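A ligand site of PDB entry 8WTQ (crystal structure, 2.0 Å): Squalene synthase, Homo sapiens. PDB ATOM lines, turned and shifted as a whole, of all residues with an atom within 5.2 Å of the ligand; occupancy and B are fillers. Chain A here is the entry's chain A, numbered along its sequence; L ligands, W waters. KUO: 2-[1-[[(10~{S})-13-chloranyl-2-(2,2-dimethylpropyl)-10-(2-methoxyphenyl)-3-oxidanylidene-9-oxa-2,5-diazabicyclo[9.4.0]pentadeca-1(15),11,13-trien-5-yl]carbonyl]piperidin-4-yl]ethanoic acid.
O2 of the ligand sits at hydrogen-bond distance from N of Ser 23 (2.9 Å).
The side-chain hydroxyl of Ser 23 lies within hydrogen-bond range of an oxygen (O2) of the ligand.
O3 of the ligand is in hydrogen-bond range of OH of Tyr 43 (2.9 Å).
The backbone carbonyl oxygen of Leu 181 sits close to the side-chain amide oxygen of Asn 185 (3.4 Å).
Ser 21 touches the ligand (O to C9, 3.5 Å).
Arg 22 touches the ligand (CB to O2, 3.4 Å).
Phe 24 touches the ligand.
CD1 of Leu 46 touches C17 of the ligand, 3.8 Å away.
Val 145 touches the ligand (O to C, 3.8 Å).
Ala 146 touches the ligand.
CG1 of Val 149 touches C18 of the ligand, at 3.6 Å.
Gly 150 touches the ligand.
Leu 153 touches the ligand (CD1 to C29, 3.5 Å).
Gly 178 touches the ligand (CA to C31, 3.8 Å).
CD1 of Leu 181 touches O5 of the ligand (3.6 Å).
Gln 182 touches the ligand (OE1 to C2, 3.5 Å).
Phe 258 touches the ligand.
CG of Pro 262 touches C22 of the ligand (3.7 Å).
Hydrophobic or aromatic side chains within 4 Å of the ligand: Phe 24, Tyr 43, Leu 46, Ala 146, Val 149, Leu 153, Leu 181, Phe 258 and Pro 262.
Within 4 Å of the ligand: Ser 21, Arg 22, Ser 23, Phe 24, Tyr 43, Leu 46, Val 145, Ala 146, Val 149, Gly 150, Leu 153, Gly 178, Leu 181, Gln 182, Phe 258 and Pro 262.
The nearest printed residue that does not touch the ligand is Cys 259 (4.1 Å).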
ATOM      1  N   THR A  20      -2.957   2.126  29.944  1.00  0.00           N
ATOM      2  CA  THR A  20      -4.172   2.862  30.272  1.00  0.00           C
ATOM      3  C   THR A  20      -5.054   3.040  29.048  1.00  0.00           C
ATOM      4  O   THR A  20      -6.261   2.875  29.163  1.00  0.00           O
ATOM      5  CB  THR A  20      -3.910   4.130  31.094  1.00  0.00           C
ATOM      6  OG1 THR A  20      -3.033   4.979  30.345  1.00  0.00           O
ATOM      7  CG2 THR A  20      -3.306   3.827  32.450  1.00  0.00           C
ATOM      8  N   SER A  21      -4.475   3.323  27.880  1.00  0.00           N
ATOM      9  CA  SER A  21      -5.300   3.628  26.712  1.00  0.00           C
ATOM     10  C   SER A  21      -5.373   2.456  25.732  1.00  0.00           C
ATOM     11  O   SER A  21      -6.082   2.512  24.730  1.00  0.00           O
ATOM     12  CB  SER A  21      -4.775   4.877  26.054  1.00  0.00           C
ATOM     13  OG  SER A  21      -3.513   4.612  25.475  1.00  0.00           O
ATOM     14  N   ARG A  22      -4.605   1.389  25.995  1.00  0.00           N
ATOM     15  CA  ARG A  22      -4.787   0.096  25.324  1.00  0.00           C
ATOM     16  C   ARG A  22      -4.693   0.232  23.806  1.00  0.00           C
ATOM     17  O   ARG A  22      -3.635   0.582  23.270  1.00  0.00           O
ATOM     18  CB  ARG A  22      -6.074  -0.601  25.798  1.00  0.00           C
ATOM     19  CG  ARG A  22      -6.134  -0.930  27.283  1.00  0.00           C
ATOM     20  CD  ARG A  22      -7.545  -1.204  27.799  1.00  0.00           C
ATOM     21  N   SER A  23      -5.792  -0.099  23.093  1.00  0.00           N
ATOM     22  CA  SER A  23      -5.729  -0.122  21.634  1.00  0.00           C
ATOM     23  C   SER A  23      -5.591   1.293  21.069  1.00  0.00           C
ATOM     24  O   SER A  23      -5.206   1.487  19.923  1.00  0.00           O
ATOM     25  CB  SER A  23      -6.923  -0.853  21.045  1.00  0.00           C
ATOM     26  OG  SER A  23      -8.097  -0.100  21.243  1.00  0.00           O
ATOM     27  N   PHE A  24      -5.873   2.309  21.898  1.00  0.00           N
ATOM     28  CA  PHE A  24      -5.792   3.697  21.452  1.00  0.00           C
ATOM     29  C   PHE A  24      -4.374   4.238  21.592  1.00  0.00           C
ATOM     30  O   PHE A  24      -4.061   5.268  21.010  1.00  0.00           O
ATOM     31  CB  PHE A  24      -6.803   4.557  22.213  1.00  0.00           C
ATOM     32  CG  PHE A  24      -7.039   5.918  21.597  1.00  0.00           C
ATOM     33  CD1 PHE A  24      -7.710   6.047  20.383  1.00  0.00           C
ATOM     34  CD2 PHE A  24      -6.607   7.081  22.253  1.00  0.00           C
ATOM     35  CE1 PHE A  24      -7.933   7.324  19.846  1.00  0.00           C
ATOM     36  CE2 PHE A  24      -6.860   8.338  21.719  1.00  0.00           C
ATOM     37  CZ  PHE A  24      -7.522   8.456  20.521  1.00  0.00           C
ATOM     38  N   VAL A  39       0.938  14.961  23.943  1.00  0.00           N
ATOM     39  CA  VAL A  39      -0.349  14.322  24.203  1.00  0.00           C
ATOM     40  C   VAL A  39      -0.197  13.149  25.180  1.00  0.00           C
ATOM     41  O   VAL A  39      -1.054  12.922  26.064  1.00  0.00           O
ATOM     42  CB  VAL A  39      -1.058  13.917  22.892  1.00  0.00           C
ATOM     43  CG1 VAL A  39      -2.263  12.994  23.112  1.00  0.00           C
ATOM     44  CG2 VAL A  39      -1.477  15.151  22.135  1.00  0.00           C
ATOM     45  N   PHE A  42      -0.019  14.584  28.579  1.00  0.00           N
ATOM     46  CA  PHE A  42      -1.282  15.166  29.001  1.00  0.00           C
ATOM     47  C   PHE A  42      -2.260  14.052  29.367  1.00  0.00           C
ATOM     48  O   PHE A  42      -3.003  14.137  30.366  1.00  0.00           O
ATOM     49  CB  PHE A  42      -1.850  16.055  27.886  1.00  0.00           C
ATOM     50  CG  PHE A  42      -3.103  16.861  28.202  1.00  0.00           C
ATOM     51  CD1 PHE A  42      -3.323  17.384  29.477  1.00  0.00           C
ATOM     52  CD2 PHE A  42      -4.040  17.131  27.211  1.00  0.00           C
ATOM     53  CE1 PHE A  42      -4.450  18.149  29.769  1.00  0.00           C
ATOM     54  CE2 PHE A  42      -5.162  17.924  27.483  1.00  0.00           C
ATOM     55  CZ  PHE A  42      -5.348  18.455  28.757  1.00  0.00           C
ATOM     56  N   TYR A  43      -2.304  13.010  28.533  1.00  0.00           N
ATOM     57  CA  TYR A  43      -3.144  11.842  28.798  1.00  0.00           C
ATOM     58  C   TYR A  43      -2.856  11.280  30.196  1.00  0.00           C
ATOM     59  O   TYR A  43      -3.788  11.062  30.968  1.00  0.00           O
ATOM     60  CB  TYR A  43      -2.966  10.757  27.726  1.00  0.00           C
ATOM     61  CG  TYR A  43      -3.972   9.628  27.795  1.00  0.00           C
ATOM     62  CD1 TYR A  43      -3.792   8.568  28.687  1.00  0.00           C
ATOM     63  CD2 TYR A  43      -5.100   9.624  27.002  1.00  0.00           C
ATOM     64  CE1 TYR A  43      -4.711   7.533  28.794  1.00  0.00           C
ATOM     65  CE2 TYR A  43      -6.022   8.601  27.083  1.00  0.00           C
ATOM     66  CZ  TYR A  43      -5.812   7.562  27.973  1.00  0.00           C
ATOM     67  OH  TYR A  43      -6.704   6.537  28.050  1.00  0.00           O
ATOM     68  N   LEU A  46      -3.903  13.571  33.084  1.00  0.00           N
ATOM     69  CA  LEU A  46      -5.357  13.547  33.242  1.00  0.00           C
ATOM     70  C   LEU A  46      -5.798  12.236  33.895  1.00  0.00           C
ATOM     71  O   LEU A  46      -6.758  12.205  34.643  1.00  0.00           O
ATOM     72  CB  LEU A  46      -6.019  13.639  31.863  1.00  0.00           C
ATOM     73  CG  LEU A  46      -5.924  15.059  31.281  1.00  0.00           C
ATOM     74  CD1 LEU A  46      -6.352  15.093  29.780  1.00  0.00           C
ATOM     75  CD2 LEU A  46      -6.764  16.010  32.139  1.00  0.00           C
ATOM     76  N   VAL A 145     -14.858  17.928  33.224  1.00  0.00           N
ATOM     77  CA  VAL A 145     -14.166  16.629  33.233  1.00  0.00           C
ATOM     78  C   VAL A 145     -13.790  16.189  31.813  1.00  0.00           C
ATOM     79  O   VAL A 145     -12.980  15.262  31.650  1.00  0.00           O
ATOM     80  CB  VAL A 145     -14.959  15.512  33.956  1.00  0.00           C
ATOM     81  CG1 VAL A 145     -15.265  15.905  35.410  1.00  0.00           C
ATOM     82  CG2 VAL A 145     -16.245  15.143  33.186  1.00  0.00           C
ATOM     83  N   ALA A 146     -14.352  16.863  30.790  1.00  0.00           N
ATOM     84  CA  ALA A 146     -14.196  16.354  29.436  1.00  0.00           C
ATOM     85  C   ALA A 146     -14.053  17.491  28.416  1.00  0.00           C
ATOM     86  O   ALA A 146     -13.197  17.413  27.532  1.00  0.00           O
ATOM     87  CB  ALA A 146     -15.375  15.464  29.093  1.00  0.00           C
ATOM     88  N   VAL A 149     -10.736  18.891  28.383  1.00  0.00           N
ATOM     89  CA  VAL A 149      -9.754  18.014  27.735  1.00  0.00           C
ATOM     90  C   VAL A 149      -9.733  18.305  26.247  1.00  0.00           C
ATOM     91  O   VAL A 149      -8.674  18.414  25.629  1.00  0.00           O
ATOM     92  CB  VAL A 149     -10.071  16.523  28.016  1.00  0.00           C
ATOM     93  CG1 VAL A 149      -9.132  15.559  27.250  1.00  0.00           C
ATOM     94  CG2 VAL A 149      -9.958  16.276  29.524  1.00  0.00           C
ATOM     95  N   GLY A 150     -10.917  18.447  25.639  1.00  0.00           N
ATOM     96  CA  GLY A 150     -10.936  18.766  24.222  1.00  0.00           C
ATOM     97  C   GLY A 150     -10.262  20.104  23.972  1.00  0.00           C
ATOM     98  O   GLY A 150      -9.549  20.276  22.988  1.00  0.00           O
ATOM     99  N   LEU A 153      -6.358  19.764  24.319  1.00  0.00           N
ATOM    100  CA  LEU A 153      -5.775  19.079  23.187  1.00  0.00           C
ATOM    101  C   LEU A 153      -5.695  20.047  22.009  1.00  0.00           C
ATOM    102  O   LEU A 153      -4.689  20.061  21.278  1.00  0.00           O
ATOM    103  CB  LEU A 153      -6.594  17.825  22.870  1.00  0.00           C
ATOM    104  CG  LEU A 153      -6.433  16.672  23.878  1.00  0.00           C
ATOM    105  CD1 LEU A 153      -7.503  15.611  23.628  1.00  0.00           C
ATOM    106  CD2 LEU A 153      -5.059  15.978  23.698  1.00  0.00           C
ATOM    107  N   MET A 177     -16.534  18.485  21.461  1.00  0.00           N
ATOM    108  CA  MET A 177     -15.831  17.220  21.212  1.00  0.00           C
ATOM    109  C   MET A 177     -15.767  16.357  22.481  1.00  0.00           C
ATOM    110  O   MET A 177     -16.020  15.146  22.466  1.00  0.00           O
ATOM    111  CB  MET A 177     -14.401  17.454  20.683  1.00  0.00           C
ATOM    112  CG  MET A 177     -14.344  18.090  19.293  1.00  0.00           C
ATOM    113  SD  MET A 177     -14.616  16.836  17.945  1.00  0.00           S
ATOM    114  CE  MET A 177     -13.092  15.907  17.978  1.00  0.00           C
ATOM    115  N   GLY A 178     -15.427  17.004  23.598  1.00  0.00           N
ATOM    116  CA  GLY A 178     -15.376  16.352  24.890  1.00  0.00           C
ATOM    117  C   GLY A 178     -16.750  15.934  25.426  1.00  0.00           C
ATOM    118  O   GLY A 178     -16.890  14.835  25.966  1.00  0.00           O
ATOM    119  N   LEU A 181     -18.254  12.728  23.753  1.00  0.00           N
ATOM    120  CA  LEU A 181     -17.725  11.479  24.282  1.00  0.00           C
ATOM    121  C   LEU A 181     -18.227  11.224  25.710  1.00  0.00           C
ATOM    122  O   LEU A 181     -18.547  10.094  26.040  1.00  0.00           O
ATOM    123  CB  LEU A 181     -16.183  11.505  24.317  1.00  0.00           C
ATOM    124  CG  LEU A 181     -15.492  11.795  22.983  1.00  0.00           C
ATOM    125  CD1 LEU A 181     -13.971  11.683  23.193  1.00  0.00           C
ATOM    126  CD2 LEU A 181     -15.963  10.791  21.920  1.00  0.00           C
ATOM    127  N   GLN A 182     -18.196  12.271  26.548  1.00  0.00           N
ATOM    128  CA  GLN A 182     -18.483  12.119  27.956  1.00  0.00           C
ATOM    129  C   GLN A 182     -19.955  11.702  28.148  1.00  0.00           C
ATOM    130  O   GLN A 182     -20.218  10.800  28.950  1.00  0.00           O
ATOM    131  CB  GLN A 182     -18.225  13.423  28.717  1.00  0.00           C
ATOM    132  CG  GLN A 182     -18.366  13.293  30.250  1.00  0.00           C
ATOM    133  CD  GLN A 182     -17.399  12.261  30.784  1.00  0.00           C
ATOM    134  OE1 GLN A 182     -16.198  12.449  30.835  1.00  0.00           O
ATOM    135  NE2 GLN A 182     -17.899  11.083  31.098  1.00  0.00           N
ATOM    136  N   ASN A 185     -20.477   8.113  27.141  1.00  0.00           N
ATOM    137  CA  ASN A 185     -19.974   7.214  28.150  1.00  0.00           C
ATOM    138  C   ASN A 185     -20.958   7.151  29.329  1.00  0.00           C
ATOM    139  O   ASN A 185     -21.324   6.078  29.751  1.00  0.00           O
ATOM    140  CB  ASN A 185     -18.596   7.657  28.671  1.00  0.00           C
ATOM    141  CG  ASN A 185     -17.519   7.434  27.628  1.00  0.00           C
ATOM    142  OD1 ASN A 185     -17.798   6.842  26.567  1.00  0.00           O
ATOM    143  ND2 ASN A 185     -16.299   7.871  27.932  1.00  0.00           N
ATOM    144  N   PHE A 258      -6.506  10.926  15.282  1.00  0.00           N
ATOM    145  CA  PHE A 258      -6.608  11.020  16.730  1.00  0.00           C
ATOM    146  C   PHE A 258      -7.975  11.537  17.151  1.00  0.00           C
ATOM    147  O   PHE A 258      -8.581  10.957  18.047  1.00  0.00           O
ATOM    148  CB  PHE A 258      -5.503  11.944  17.266  1.00  0.00           C
ATOM    149  CG  PHE A 258      -5.546  12.215  18.760  1.00  0.00           C
ATOM    150  CD1 PHE A 258      -5.361  11.189  19.681  1.00  0.00           C
ATOM    151  CD2 PHE A 258      -5.790  13.486  19.238  1.00  0.00           C
ATOM    152  CE1 PHE A 258      -5.380  11.438  21.047  1.00  0.00           C
ATOM    153  CE2 PHE A 258      -5.780  13.741  20.611  1.00  0.00           C
ATOM    154  CZ  PHE A 258      -5.561  12.719  21.507  1.00  0.00           C
ATOM    155  N   CYS A 259      -8.450  12.628  16.531  1.00  0.00           N
ATOM    156  CA  CYS A 259      -9.700  13.236  16.963  1.00  0.00           C
ATOM    157  C   CYS A 259     -10.927  12.470  16.447  1.00  0.00           C
ATOM    158  O   CYS A 259     -11.958  12.373  17.121  1.00  0.00           O
ATOM    159  CB  CYS A 259      -9.794  14.704  16.533  1.00  0.00           C
ATOM    160  SG  CYS A 259      -8.554  15.751  17.347  1.00  0.00           S
ATOM    161  N   PRO A 262     -12.364   8.478  18.215  1.00  0.00           N
ATOM    162  CA  PRO A 262     -13.299   8.397  19.343  1.00  0.00           C
ATOM    163  C   PRO A 262     -14.695   8.872  18.943  1.00  0.00           C
ATOM    164  O   PRO A 262     -15.698   8.372  19.462  1.00  0.00           O
ATOM    165  CB  PRO A 262     -12.634   9.263  20.424  1.00  0.00           C
ATOM    166  CG  PRO A 262     -11.157   9.321  19.991  1.00  0.00           C
ATOM    167  CD  PRO A 262     -11.202   9.384  18.474  1.00  0.00           C
HETATM  168  N1  KUO L   1      -9.827   7.245  25.889  1.00  0.00           N
HETATM  169  C2  KUO L   1     -14.479  12.201  27.831  1.00  0.00           C
HETATM  170  C3  KUO L   1     -12.938  10.670  29.159  1.00  0.00           C
HETATM  171  C6  KUO L   1      -9.702   8.493  26.726  1.00  0.00           C
HETATM  172  C7  KUO L   1      -9.894   6.118  26.719  1.00  0.00           C
HETATM  173  C9  KUO L   1      -9.274   2.526  26.067  1.00  0.00           C
HETATM  174  C10 KUO L   1     -10.164   2.371  24.800  1.00  0.00           C
HETATM  175  C20 KUO L   1      -9.387  11.771  25.545  1.00  0.00           C
HETATM  176  C21 KUO L   1     -10.156  11.355  24.314  1.00  0.00           C
HETATM  177  C25 KUO L   1      -9.950  12.285  23.136  1.00  0.00           C
HETATM  178  C26 KUO L   1      -9.155  11.911  22.053  1.00  0.00           C
HETATM  179  C27 KUO L   1      -9.044  12.830  20.966  1.00  0.00           C
HETATM  180  C28 KUO L   1      -9.680  14.089  20.957  1.00  0.00           C
HETATM  181  C29 KUO L   1     -10.467  14.457  22.107  1.00  0.00           C
HETATM  182  C30 KUO L   1     -10.565  13.561  23.179  1.00  0.00           C
HETATM  183  C31 KUO L   1     -11.860  15.036  24.619  1.00  0.00           C
HETATM  184  O2  KUO L   1      -8.579  -0.764  23.576  1.00  0.00           O
HETATM  185  C12 KUO L   1      -9.464  -0.033  24.297  1.00  0.00           C
HETATM  186  O1  KUO L   1     -10.007  -0.417  25.341  1.00  0.00           O
HETATM  187  C11 KUO L   1      -9.671   1.389  23.729  1.00  0.00           C
HETATM  188  C8  KUO L   1      -9.855   3.680  26.952  1.00  0.00           C
HETATM  189  C13 KUO L   1     -10.610   3.717  24.125  1.00  0.00           C
HETATM  190  C14 KUO L   1     -11.199   4.730  25.144  1.00  0.00           C
HETATM  191  N2  KUO L   1     -10.217   4.897  26.196  1.00  0.00           N
HETATM  192  O3  KUO L   1      -9.628   6.173  27.944  1.00  0.00           O
HETATM  193  C5  KUO L   1     -11.022   9.236  26.921  1.00  0.00           C
HETATM  194  O   KUO L   1     -12.057   8.569  26.892  1.00  0.00           O
HETATM  195  N   KUO L   1     -11.011  10.599  27.007  1.00  0.00           N
HETATM  196  C4  KUO L   1     -12.283  11.344  26.788  1.00  0.00           C
HETATM  197  C1  KUO L   1     -12.989  11.801  28.129  1.00  0.00           C
HETATM  198  C   KUO L   1     -12.178  13.008  28.705  1.00  0.00           C
HETATM  199  C15 KUO L   1      -9.743  11.253  26.795  1.00  0.00           C
HETATM  200  C16 KUO L   1      -8.917  11.523  27.902  1.00  0.00           C
HETATM  201  C17 KUO L   1      -7.646  12.174  27.789  1.00  0.00           C
HETATM  202  C18 KUO L   1      -7.240  12.534  26.518  1.00  0.00           C
HETATM  203 CL   KUO L   1      -5.732  13.313  26.317  1.00  0.00          CL
HETATM  204  C19 KUO L   1      -8.066  12.291  25.401  1.00  0.00           C
HETATM  205  C24 KUO L   1      -9.070   7.285  24.602  1.00  0.00           C
HETATM  206  C23 KUO L   1      -9.982   7.691  23.404  1.00  0.00           C
HETATM  207  C22 KUO L   1     -10.724   9.030  23.605  1.00  0.00           C
HETATM  208  O4  KUO L   1      -9.772  10.020  23.978  1.00  0.00           O
HETATM  209  O5  KUO L   1     -11.277  13.771  24.336  1.00  0.00           O
HETATM  210  O   HOH W   1     -12.334  12.799  19.860  1.00  0.00           O
HETATM  211  O   HOH W   2      -6.566  10.392  30.356  1.00  0.00           O
HETATM  212  O   HOH W   3      -9.418  11.946  31.065  1.00  0.00           O
HETATM  213  O   HOH W   4      -8.315  -3.559  24.590  1.00  0.00           O
